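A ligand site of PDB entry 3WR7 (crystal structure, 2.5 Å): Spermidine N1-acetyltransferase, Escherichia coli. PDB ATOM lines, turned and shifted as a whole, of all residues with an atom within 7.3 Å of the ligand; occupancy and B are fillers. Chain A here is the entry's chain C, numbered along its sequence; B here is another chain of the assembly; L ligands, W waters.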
ATOM      1  N   TYR A  44     -15.057  25.127  38.379  1.00  0.00           N
ATOM      2  CA  TYR A  44     -13.906  25.079  37.511  1.00  0.00           C
ATOM      3  C   TYR A  44     -13.193  23.711  37.696  1.00  0.00           C
ATOM      4  O   TYR A  44     -12.937  23.013  36.713  1.00  0.00           O
ATOM      5  CB  TYR A  44     -12.997  26.222  37.814  1.00  0.00           C
ATOM      6  CG  TYR A  44     -11.743  26.274  36.972  1.00  0.00           C
ATOM      7  CD1 TYR A  44     -11.757  26.837  35.658  1.00  0.00           C
ATOM      8  CD2 TYR A  44     -10.524  25.818  37.496  1.00  0.00           C
ATOM      9  CE1 TYR A  44     -10.609  26.907  34.906  1.00  0.00           C
ATOM     10  CE2 TYR A  44      -9.355  25.907  36.754  1.00  0.00           C
ATOM     11  CZ  TYR A  44      -9.399  26.409  35.456  1.00  0.00           C
ATOM     12  OH  TYR A  44      -8.239  26.443  34.760  1.00  0.00           O
ATOM     13  N   HIS A  47     -14.774  20.777  36.113  1.00  0.00           N
ATOM     14  CA  HIS A  47     -14.781  20.700  34.677  1.00  0.00           C
ATOM     15  C   HIS A  47     -13.404  20.569  33.954  1.00  0.00           C
ATOM     16  O   HIS A  47     -13.360  20.551  32.727  1.00  0.00           O
ATOM     17  CB  HIS A  47     -15.614  21.836  34.101  1.00  0.00           C
ATOM     18  CG  HIS A  47     -17.093  21.602  34.218  1.00  0.00           C
ATOM     19  ND1 HIS A  47     -17.851  22.145  35.230  1.00  0.00           N
ATOM     20  CD2 HIS A  47     -17.939  20.865  33.448  1.00  0.00           C
ATOM     21  CE1 HIS A  47     -19.114  21.760  35.077  1.00  0.00           C
ATOM     22  NE2 HIS A  47     -19.193  20.964  34.020  1.00  0.00           N
ATOM     23  N   ILE A  48     -12.330  20.401  34.719  1.00  0.00           N
ATOM     24  CA  ILE A  48     -10.970  20.493  34.224  1.00  0.00           C
ATOM     25  C   ILE A  48     -10.806  19.543  33.026  1.00  0.00           C
ATOM     26  O   ILE A  48     -10.248  19.938  31.998  1.00  0.00           O
ATOM     27  CB  ILE A  48      -9.931  20.125  35.351  1.00  0.00           C
ATOM     28  CG1 ILE A  48      -9.890  21.213  36.405  1.00  0.00           C
ATOM     29  CG2 ILE A  48      -8.529  19.917  34.769  1.00  0.00           C
ATOM     30  CD1 ILE A  48      -8.907  20.916  37.609  1.00  0.00           C
ATOM     31  N   HIS A  49     -11.305  18.312  33.180  1.00  0.00           N
ATOM     32  CA  HIS A  49     -11.224  17.290  32.172  1.00  0.00           C
ATOM     33  C   HIS A  49     -12.475  17.214  31.321  1.00  0.00           C
ATOM     34  O   HIS A  49     -12.661  16.241  30.591  1.00  0.00           O
ATOM     35  CB  HIS A  49     -10.941  15.919  32.818  1.00  0.00           C
ATOM     36  CG  HIS A  49      -9.691  15.935  33.648  1.00  0.00           C
ATOM     37  ND1 HIS A  49      -8.435  15.945  33.080  1.00  0.00           N
ATOM     38  CD2 HIS A  49      -9.508  16.091  34.978  1.00  0.00           C
ATOM     39  CE1 HIS A  49      -7.538  16.097  34.045  1.00  0.00           C
ATOM     40  NE2 HIS A  49      -8.165  16.190  35.198  1.00  0.00           N
ATOM     41  N   ASP A  50     -13.340  18.211  31.397  1.00  0.00           N
ATOM     42  CA  ASP A  50     -14.568  18.146  30.620  1.00  0.00           C
ATOM     43  C   ASP A  50     -14.190  18.513  29.170  1.00  0.00           C
ATOM     44  O   ASP A  50     -13.817  19.663  28.909  1.00  0.00           O
ATOM     45  CB  ASP A  50     -15.591  19.143  31.175  1.00  0.00           C
ATOM     46  CG  ASP A  50     -16.909  19.107  30.409  1.00  0.00           C
ATOM     47  OD1 ASP A  50     -17.110  18.254  29.511  1.00  0.00           O
ATOM     48  OD2 ASP A  50     -17.776  19.922  30.703  1.00  0.00           O
ATOM     49  N   GLN A  51     -14.223  17.550  28.261  1.00  0.00           N
ATOM     50  CA  GLN A  51     -13.783  17.832  26.862  1.00  0.00           C
ATOM     51  C   GLN A  51     -14.884  18.561  26.034  1.00  0.00           C
ATOM     52  O   GLN A  51     -14.651  18.987  24.874  1.00  0.00           O
ATOM     53  CB  GLN A  51     -13.293  16.565  26.113  1.00  0.00           C
ATOM     54  CG  GLN A  51     -11.960  15.883  26.535  1.00  0.00           C
ATOM     55  CD  GLN A  51     -10.835  16.800  27.037  1.00  0.00           C
ATOM     56  OE1 GLN A  51     -10.402  17.796  26.373  1.00  0.00           O
ATOM     57  NE2 GLN A  51     -10.314  16.451  28.227  1.00  0.00           N
ATOM     58  N   SER A  52     -16.054  18.748  26.652  1.00  0.00           N
ATOM     59  CA  SER A  52     -17.177  19.420  26.001  1.00  0.00           C
ATOM     60  C   SER A  52     -17.135  20.949  26.075  1.00  0.00           C
ATOM     61  O   SER A  52     -18.079  21.633  25.608  1.00  0.00           O
ATOM     62  CB  SER A  52     -18.500  18.902  26.546  1.00  0.00           C
ATOM     63  OG  SER A  52     -18.942  19.759  27.581  1.00  0.00           O
ATOM     64  N   GLU A  53     -16.054  21.534  26.574  1.00  0.00           N
ATOM     65  CA  GLU A  53     -15.945  22.998  26.580  1.00  0.00           C
ATOM     66  C   GLU A  53     -14.494  23.454  26.443  1.00  0.00           C
ATOM     67  O   GLU A  53     -13.551  22.651  26.489  1.00  0.00           O
ATOM     68  CB  GLU A  53     -16.600  23.574  27.871  1.00  0.00           C
ATOM     69  CG  GLU A  53     -15.712  23.470  29.124  1.00  0.00           C
ATOM     70  CD  GLU A  53     -16.356  23.965  30.453  1.00  0.00           C
ATOM     71  OE1 GLU A  53     -17.572  24.345  30.472  1.00  0.00           O
ATOM     72  OE2 GLU A  53     -15.628  23.960  31.490  1.00  0.00           O
ATOM     73  N   ARG A  54     -14.298  24.749  26.231  1.00  0.00           N
ATOM     74  CA  ARG A  54     -12.978  25.329  26.260  1.00  0.00           C
ATOM     75  C   ARG A  54     -13.285  26.740  26.591  1.00  0.00           C
ATOM     76  O   ARG A  54     -14.080  27.379  25.896  1.00  0.00           O
ATOM     77  CB  ARG A  54     -12.330  25.391  24.879  1.00  0.00           C
ATOM     78  CG  ARG A  54     -12.086  24.061  24.207  1.00  0.00           C
ATOM     79  CD  ARG A  54     -10.876  23.397  24.812  1.00  0.00           C
ATOM     80  NE  ARG A  54     -10.554  22.196  24.079  1.00  0.00           N
ATOM     81  CZ  ARG A  54     -11.289  21.104  24.065  1.00  0.00           C
ATOM     82  NH1 ARG A  54     -10.895  20.094  23.315  1.00  0.00           N
ATOM     83  NH2 ARG A  54     -12.428  21.008  24.774  1.00  0.00           N
ATOM     84  N   ARG A  55     -12.650  27.215  27.664  1.00  0.00           N
ATOM     85  CA  ARG A  55     -12.811  28.519  28.160  1.00  0.00           C
ATOM     86  C   ARG A  55     -11.520  29.274  27.941  1.00  0.00           C
ATOM     87  O   ARG A  55     -10.460  28.762  28.284  1.00  0.00           O
ATOM     88  CB  ARG A  55     -13.053  28.425  29.668  1.00  0.00           C
ATOM     89  CG  ARG A  55     -14.382  27.851  30.106  1.00  0.00           C
ATOM     90  CD  ARG A  55     -14.859  28.798  31.230  1.00  0.00           C
ATOM     91  NE  ARG A  55     -15.373  28.147  32.414  1.00  0.00           N
ATOM     92  CZ  ARG A  55     -15.745  28.772  33.530  1.00  0.00           C
ATOM     93  NH1 ARG A  55     -15.673  30.091  33.663  1.00  0.00           N
ATOM     94  NH2 ARG A  55     -16.228  28.038  34.541  1.00  0.00           N
ATOM     95  N   TYR A 106     -10.861  29.185  16.149  1.00  0.00           N
ATOM     96  CA  TYR A 106     -10.628  28.014  16.968  1.00  0.00           C
ATOM     97  C   TYR A 106     -11.623  26.897  16.748  1.00  0.00           C
ATOM     98  O   TYR A 106     -11.236  25.727  16.557  1.00  0.00           O
ATOM     99  CB  TYR A 106     -10.466  28.385  18.437  1.00  0.00           C
ATOM    100  CG  TYR A 106      -9.651  27.351  19.235  1.00  0.00           C
ATOM    101  CD1 TYR A 106     -10.236  26.156  19.676  1.00  0.00           C
ATOM    102  CD2 TYR A 106      -8.313  27.583  19.537  1.00  0.00           C
ATOM    103  CE1 TYR A 106      -9.534  25.210  20.390  1.00  0.00           C
ATOM    104  CE2 TYR A 106      -7.581  26.622  20.246  1.00  0.00           C
ATOM    105  CZ  TYR A 106      -8.207  25.440  20.671  1.00  0.00           C
ATOM    106  OH  TYR A 106      -7.505  24.499  21.393  1.00  0.00           O
ATOM    107  N   ASP B  20       2.986  23.896  25.468  1.00  0.00           N
ATOM    108  CA  ASP B  20       1.790  23.209  25.110  1.00  0.00           C
ATOM    109  C   ASP B  20       0.670  24.191  24.656  1.00  0.00           C
ATOM    110  O   ASP B  20      -0.351  23.765  24.127  1.00  0.00           O
ATOM    111  CB  ASP B  20       1.362  22.313  26.277  1.00  0.00           C
ATOM    112  CG  ASP B  20       2.024  20.886  26.254  1.00  0.00           C
ATOM    113  OD1 ASP B  20       2.965  20.586  25.460  1.00  0.00           O
ATOM    114  OD2 ASP B  20       1.581  20.040  27.085  1.00  0.00           O
ATOM    115  N   MET B  26       2.947  23.201  18.682  1.00  0.00           N
ATOM    116  CA  MET B  26       2.101  22.020  18.906  1.00  0.00           C
ATOM    117  C   MET B  26       1.615  21.375  17.647  1.00  0.00           C
ATOM    118  O   MET B  26       1.330  20.174  17.653  1.00  0.00           O
ATOM    119  CB  MET B  26       0.895  22.371  19.789  1.00  0.00           C
ATOM    120  CG  MET B  26       1.215  22.486  21.278  1.00  0.00           C
ATOM    121  SD  MET B  26       1.803  20.987  22.070  1.00  0.00           S
ATOM    122  CE  MET B  26       3.470  21.472  22.469  1.00  0.00           C
ATOM    123  N   PHE B  30       0.709  17.201  16.267  1.00  0.00           N
ATOM    124  CA  PHE B  30      -0.691  16.974  15.917  1.00  0.00           C
ATOM    125  C   PHE B  30      -1.563  17.144  17.165  1.00  0.00           C
ATOM    126  O   PHE B  30      -2.429  16.327  17.483  1.00  0.00           O
ATOM    127  CB  PHE B  30      -0.859  15.620  15.234  1.00  0.00           C
ATOM    128  CG  PHE B  30       0.005  15.481  14.038  1.00  0.00           C
ATOM    129  CD1 PHE B  30      -0.322  16.130  12.852  1.00  0.00           C
ATOM    130  CD2 PHE B  30       1.201  14.763  14.101  1.00  0.00           C
ATOM    131  CE1 PHE B  30       0.507  16.061  11.731  1.00  0.00           C
ATOM    132  CE2 PHE B  30       2.019  14.667  12.974  1.00  0.00           C
ATOM    133  CZ  PHE B  30       1.662  15.325  11.785  1.00  0.00           C
ATOM    134  N   GLU B  31      -1.276  18.218  17.886  1.00  0.00           N
ATOM    135  CA  GLU B  31      -1.712  18.312  19.265  1.00  0.00           C
ATOM    136  C   GLU B  31      -2.439  19.626  19.431  1.00  0.00           C
ATOM    137  O   GLU B  31      -1.888  20.688  19.156  1.00  0.00           O
ATOM    138  CB  GLU B  31      -0.490  18.211  20.192  1.00  0.00           C
ATOM    139  CG  GLU B  31      -0.816  17.973  21.640  1.00  0.00           C
ATOM    140  CD  GLU B  31      -1.142  16.528  21.917  1.00  0.00           C
ATOM    141  OE1 GLU B  31      -0.206  15.704  22.025  1.00  0.00           O
ATOM    142  OE2 GLU B  31      -2.342  16.211  22.025  1.00  0.00           O
ATOM    143  N   GLU B  32      -3.681  19.542  19.879  1.00  0.00           N
ATOM    144  CA  GLU B  32      -4.499  20.716  20.067  1.00  0.00           C
ATOM    145  C   GLU B  32      -3.774  21.679  20.998  1.00  0.00           C
ATOM    146  O   GLU B  32      -3.416  21.299  22.121  1.00  0.00           O
ATOM    147  CB  GLU B  32      -5.870  20.297  20.624  1.00  0.00           C
ATOM    148  CG  GLU B  32      -6.700  21.490  20.977  1.00  0.00           C
ATOM    149  CD  GLU B  32      -7.984  21.177  21.664  1.00  0.00           C
ATOM    150  OE1 GLU B  32      -8.375  20.012  21.748  1.00  0.00           O
ATOM    151  OE2 GLU B  32      -8.612  22.136  22.128  1.00  0.00           O
ATOM    152  N   PRO B  33      -3.509  22.920  20.544  1.00  0.00           N
ATOM    153  CA  PRO B  33      -2.709  23.881  21.354  1.00  0.00           C
ATOM    154  C   PRO B  33      -3.570  24.547  22.472  1.00  0.00           C
ATOM    155  O   PRO B  33      -3.596  25.823  22.672  1.00  0.00           O
ATOM    156  CB  PRO B  33      -2.293  24.929  20.318  1.00  0.00           C
ATOM    157  CG  PRO B  33      -3.449  24.952  19.341  1.00  0.00           C
ATOM    158  CD  PRO B  33      -3.941  23.507  19.261  1.00  0.00           C
ATOM    159  N   TYR B  34      -4.267  23.710  23.228  1.00  0.00           N
ATOM    160  CA  TYR B  34      -4.958  24.262  24.383  1.00  0.00           C
ATOM    161  C   TYR B  34      -4.642  23.437  25.608  1.00  0.00           C
ATOM    162  O   TYR B  34      -4.905  22.246  25.630  1.00  0.00           O
ATOM    163  CB  TYR B  34      -6.482  24.272  24.117  1.00  0.00           C
ATOM    164  CG  TYR B  34      -7.315  24.860  25.222  1.00  0.00           C
ATOM    165  CD1 TYR B  34      -7.537  24.140  26.458  1.00  0.00           C
ATOM    166  CD2 TYR B  34      -7.917  26.134  25.054  1.00  0.00           C
ATOM    167  CE1 TYR B  34      -8.334  24.680  27.485  1.00  0.00           C
ATOM    168  CE2 TYR B  34      -8.745  26.678  26.068  1.00  0.00           C
ATOM    169  CZ  TYR B  34      -8.948  25.947  27.286  1.00  0.00           C
ATOM    170  OH  TYR B  34      -9.707  26.479  28.280  1.00  0.00           O
ATOM    171  N   GLU B  35      -4.165  24.086  26.664  1.00  0.00           N
ATOM    172  CA  GLU B  35      -4.015  23.370  27.936  1.00  0.00           C
ATOM    173  C   GLU B  35      -3.967  24.238  29.185  1.00  0.00           C
ATOM    174  O   GLU B  35      -2.966  24.996  29.415  1.00  0.00           O
ATOM    175  CB  GLU B  35      -2.767  22.514  27.869  1.00  0.00           C
ATOM    176  CG  GLU B  35      -2.379  21.779  29.105  1.00  0.00           C
ATOM    177  CD  GLU B  35      -1.316  20.743  28.771  1.00  0.00           C
ATOM    178  OE1 GLU B  35      -0.136  21.127  28.847  1.00  0.00           O
ATOM    179  OE2 GLU B  35      -1.668  19.601  28.379  1.00  0.00           O
ATOM    180  N   ALA B  36      -4.981  24.077  30.034  1.00  0.00           N
ATOM    181  CA  ALA B  36      -4.953  24.783  31.326  1.00  0.00           C
ATOM    182  C   ALA B  36      -3.923  24.002  32.167  1.00  0.00           C
ATOM    183  O   ALA B  36      -3.880  22.771  32.115  1.00  0.00           O
ATOM    184  CB  ALA B  36      -6.345  24.769  31.986  1.00  0.00           C
ATOM    185  N   GLU B  39      -4.969  21.084  34.149  1.00  0.00           N
ATOM    186  CA  GLU B  39      -5.150  19.816  33.378  1.00  0.00           C
ATOM    187  C   GLU B  39      -3.818  19.089  33.157  1.00  0.00           C
ATOM    188  O   GLU B  39      -3.775  17.863  33.114  1.00  0.00           O
ATOM    189  CB  GLU B  39      -5.762  20.045  31.997  1.00  0.00           C
ATOM    190  CG  GLU B  39      -6.357  18.762  31.364  1.00  0.00           C
ATOM    191  CD  GLU B  39      -6.705  18.870  29.856  1.00  0.00           C
ATOM    192  OE1 GLU B  39      -6.471  19.934  29.231  1.00  0.00           O
ATOM    193  OE2 GLU B  39      -7.233  17.860  29.321  1.00  0.00           O
ATOM    194  N   LEU B  43      -2.694  15.420  34.629  1.00  0.00           N
ATOM    195  CA  LEU B  43      -2.518  14.266  33.768  1.00  0.00           C
ATOM    196  C   LEU B  43      -1.109  13.782  34.051  1.00  0.00           C
ATOM    197  O   LEU B  43      -0.845  12.592  34.021  1.00  0.00           O
ATOM    198  CB  LEU B  43      -2.803  14.581  32.269  1.00  0.00           C
ATOM    199  CG  LEU B  43      -4.276  14.749  31.761  1.00  0.00           C
ATOM    200  CD1 LEU B  43      -4.353  14.886  30.256  1.00  0.00           C
ATOM    201  CD2 LEU B  43      -5.229  13.628  32.236  1.00  0.00           C
HETATM  202  N1  LIG L   1      -3.339  18.529  24.105  1.00  0.00           N
HETATM  203  C1  LIG L   1      -4.667  18.097  24.525  1.00  0.00           C
HETATM  204  C2  LIG L   1      -5.371  19.354  24.997  1.00  0.00           C
HETATM  205  C3  LIG L   1      -6.877  19.223  25.147  1.00  0.00           C
HETATM  206  C4  LIG L   1      -7.279  20.334  26.117  1.00  0.00           C
HETATM  207  N2  LIG L   1      -8.492  19.997  26.839  1.00  0.00           N
HETATM  208  C5  LIG L   1      -9.218  21.066  27.522  1.00  0.00           C
HETATM  209  C6  LIG L   1     -10.260  20.546  28.513  1.00  0.00           C
HETATM  210  C7  LIG L   1     -10.862  21.733  29.270  1.00  0.00           C
HETATM  211  N3  LIG L   1     -12.048  21.278  29.933  1.00  0.00           N
HETATM  212  O   HOH W   1      -8.897  22.123  31.843  1.00  0.00           O
HETATM  213  O   HOH W   2     -13.020  23.436  31.298  1.00  0.00           O
HETATM  214  O   HOH W   3      -6.881  22.401  29.656  1.00  0.00           O
HETATM  215  O   HOH W   4      -1.353  21.216  23.911  1.00  0.00           O
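A nitrogen (N2) of the ligand is in salt-bridge range of the side-chain carboxylate (OE1) of Glu 39 of chain B (3.1 Å).
O of Asp 50 sits at hydrogen-bond distance from N3 of the ligand, at 2.6 Å.
A nitrogen (N1) of the ligand is in salt-bridge range of the side-chain carboxylate (OE2) of Glu 31 of chain B.
O of Ile 48 is in hydrogen-bond range of N3 of the ligand (3.0 Å).
A nitrogen (N2) of the ligand lies within hydrogen-bond range of the side-chain amide oxygen (OE1) of Gln 51 (3.0 Å).
N3 of the ligand lies within hydrogen-bond range of O of His 47.
O of Glu 32 of chain B is in hydrogen-bond range of N1 of the ligand (3.4 Å).
The guanidinium group of Arg 54 is in hydrogen-bond range of the backbone carbonyl oxygen of Gln 51, 3.0 Å away.
OH of Tyr 34 of chain B is in hydrogen-bond range of O of Arg 55 (2.4 Å).
The side-chain hydroxyl (OH) of Tyr 106 lies within hydrogen-bond range of the side-chain carboxylate (OE2) of Glu 32 of chain B, 2.7 Å away.
NE of Arg 54 is in salt-bridge range of OE2 of Glu 32 of chain B (2.8 Å).
The side-chain carboxylate (OD1) of Asp 50 lies within hydrogen-bond range of the side-chain hydroxyl (OG) of Ser 52, at 3.1 Å.
O of His 49 is in hydrogen-bond range of NE2 of Gln 51, at 3.3 Å.
Merely in contact with the ligand: Tyr 34 of chain B (3.0 Å), Arg 54 (3.9 Å) and Glu 53 (3.98 Å).
Within 4 Å of the ligand: His 47, Ile 48, Asp 50, Gln 51, Glu 53, Arg 54, Glu 31 of chain B, Glu 32 of chain B, Tyr 34 of chain B and Glu 39 of chain B.
Along chain A the residues within 4 Å of the ligand span positions 47 to 54.
The nearest printed residue that does not touch the ligand is His 49 (4.3 Å).
Water W2 lies within hydrogen-bond range of the side-chain carboxylate of Glu 53 (2.7 Å), a nitrogen (N3) of the ligand (2.7 Å) and the backbone carbonyl oxygen of His 47 (3.2 Å).
Water W4 lies within hydrogen-bond range of the backbone carbonyl oxygen of Glu 32 of chain B (2.7 Å), the backbone carbonyl oxygen of Asp 20 of chain B (2.7 Å) and a nitrogen (N1) of the ligand (3.3 Å).
Water W3 lies within hydrogen-bond range of the side-chain carboxylate (OE1) of Glu 39 of chain B (2.5 Å) and the backbone NH (N) of Ala 36 of chain B (2.6 Å).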
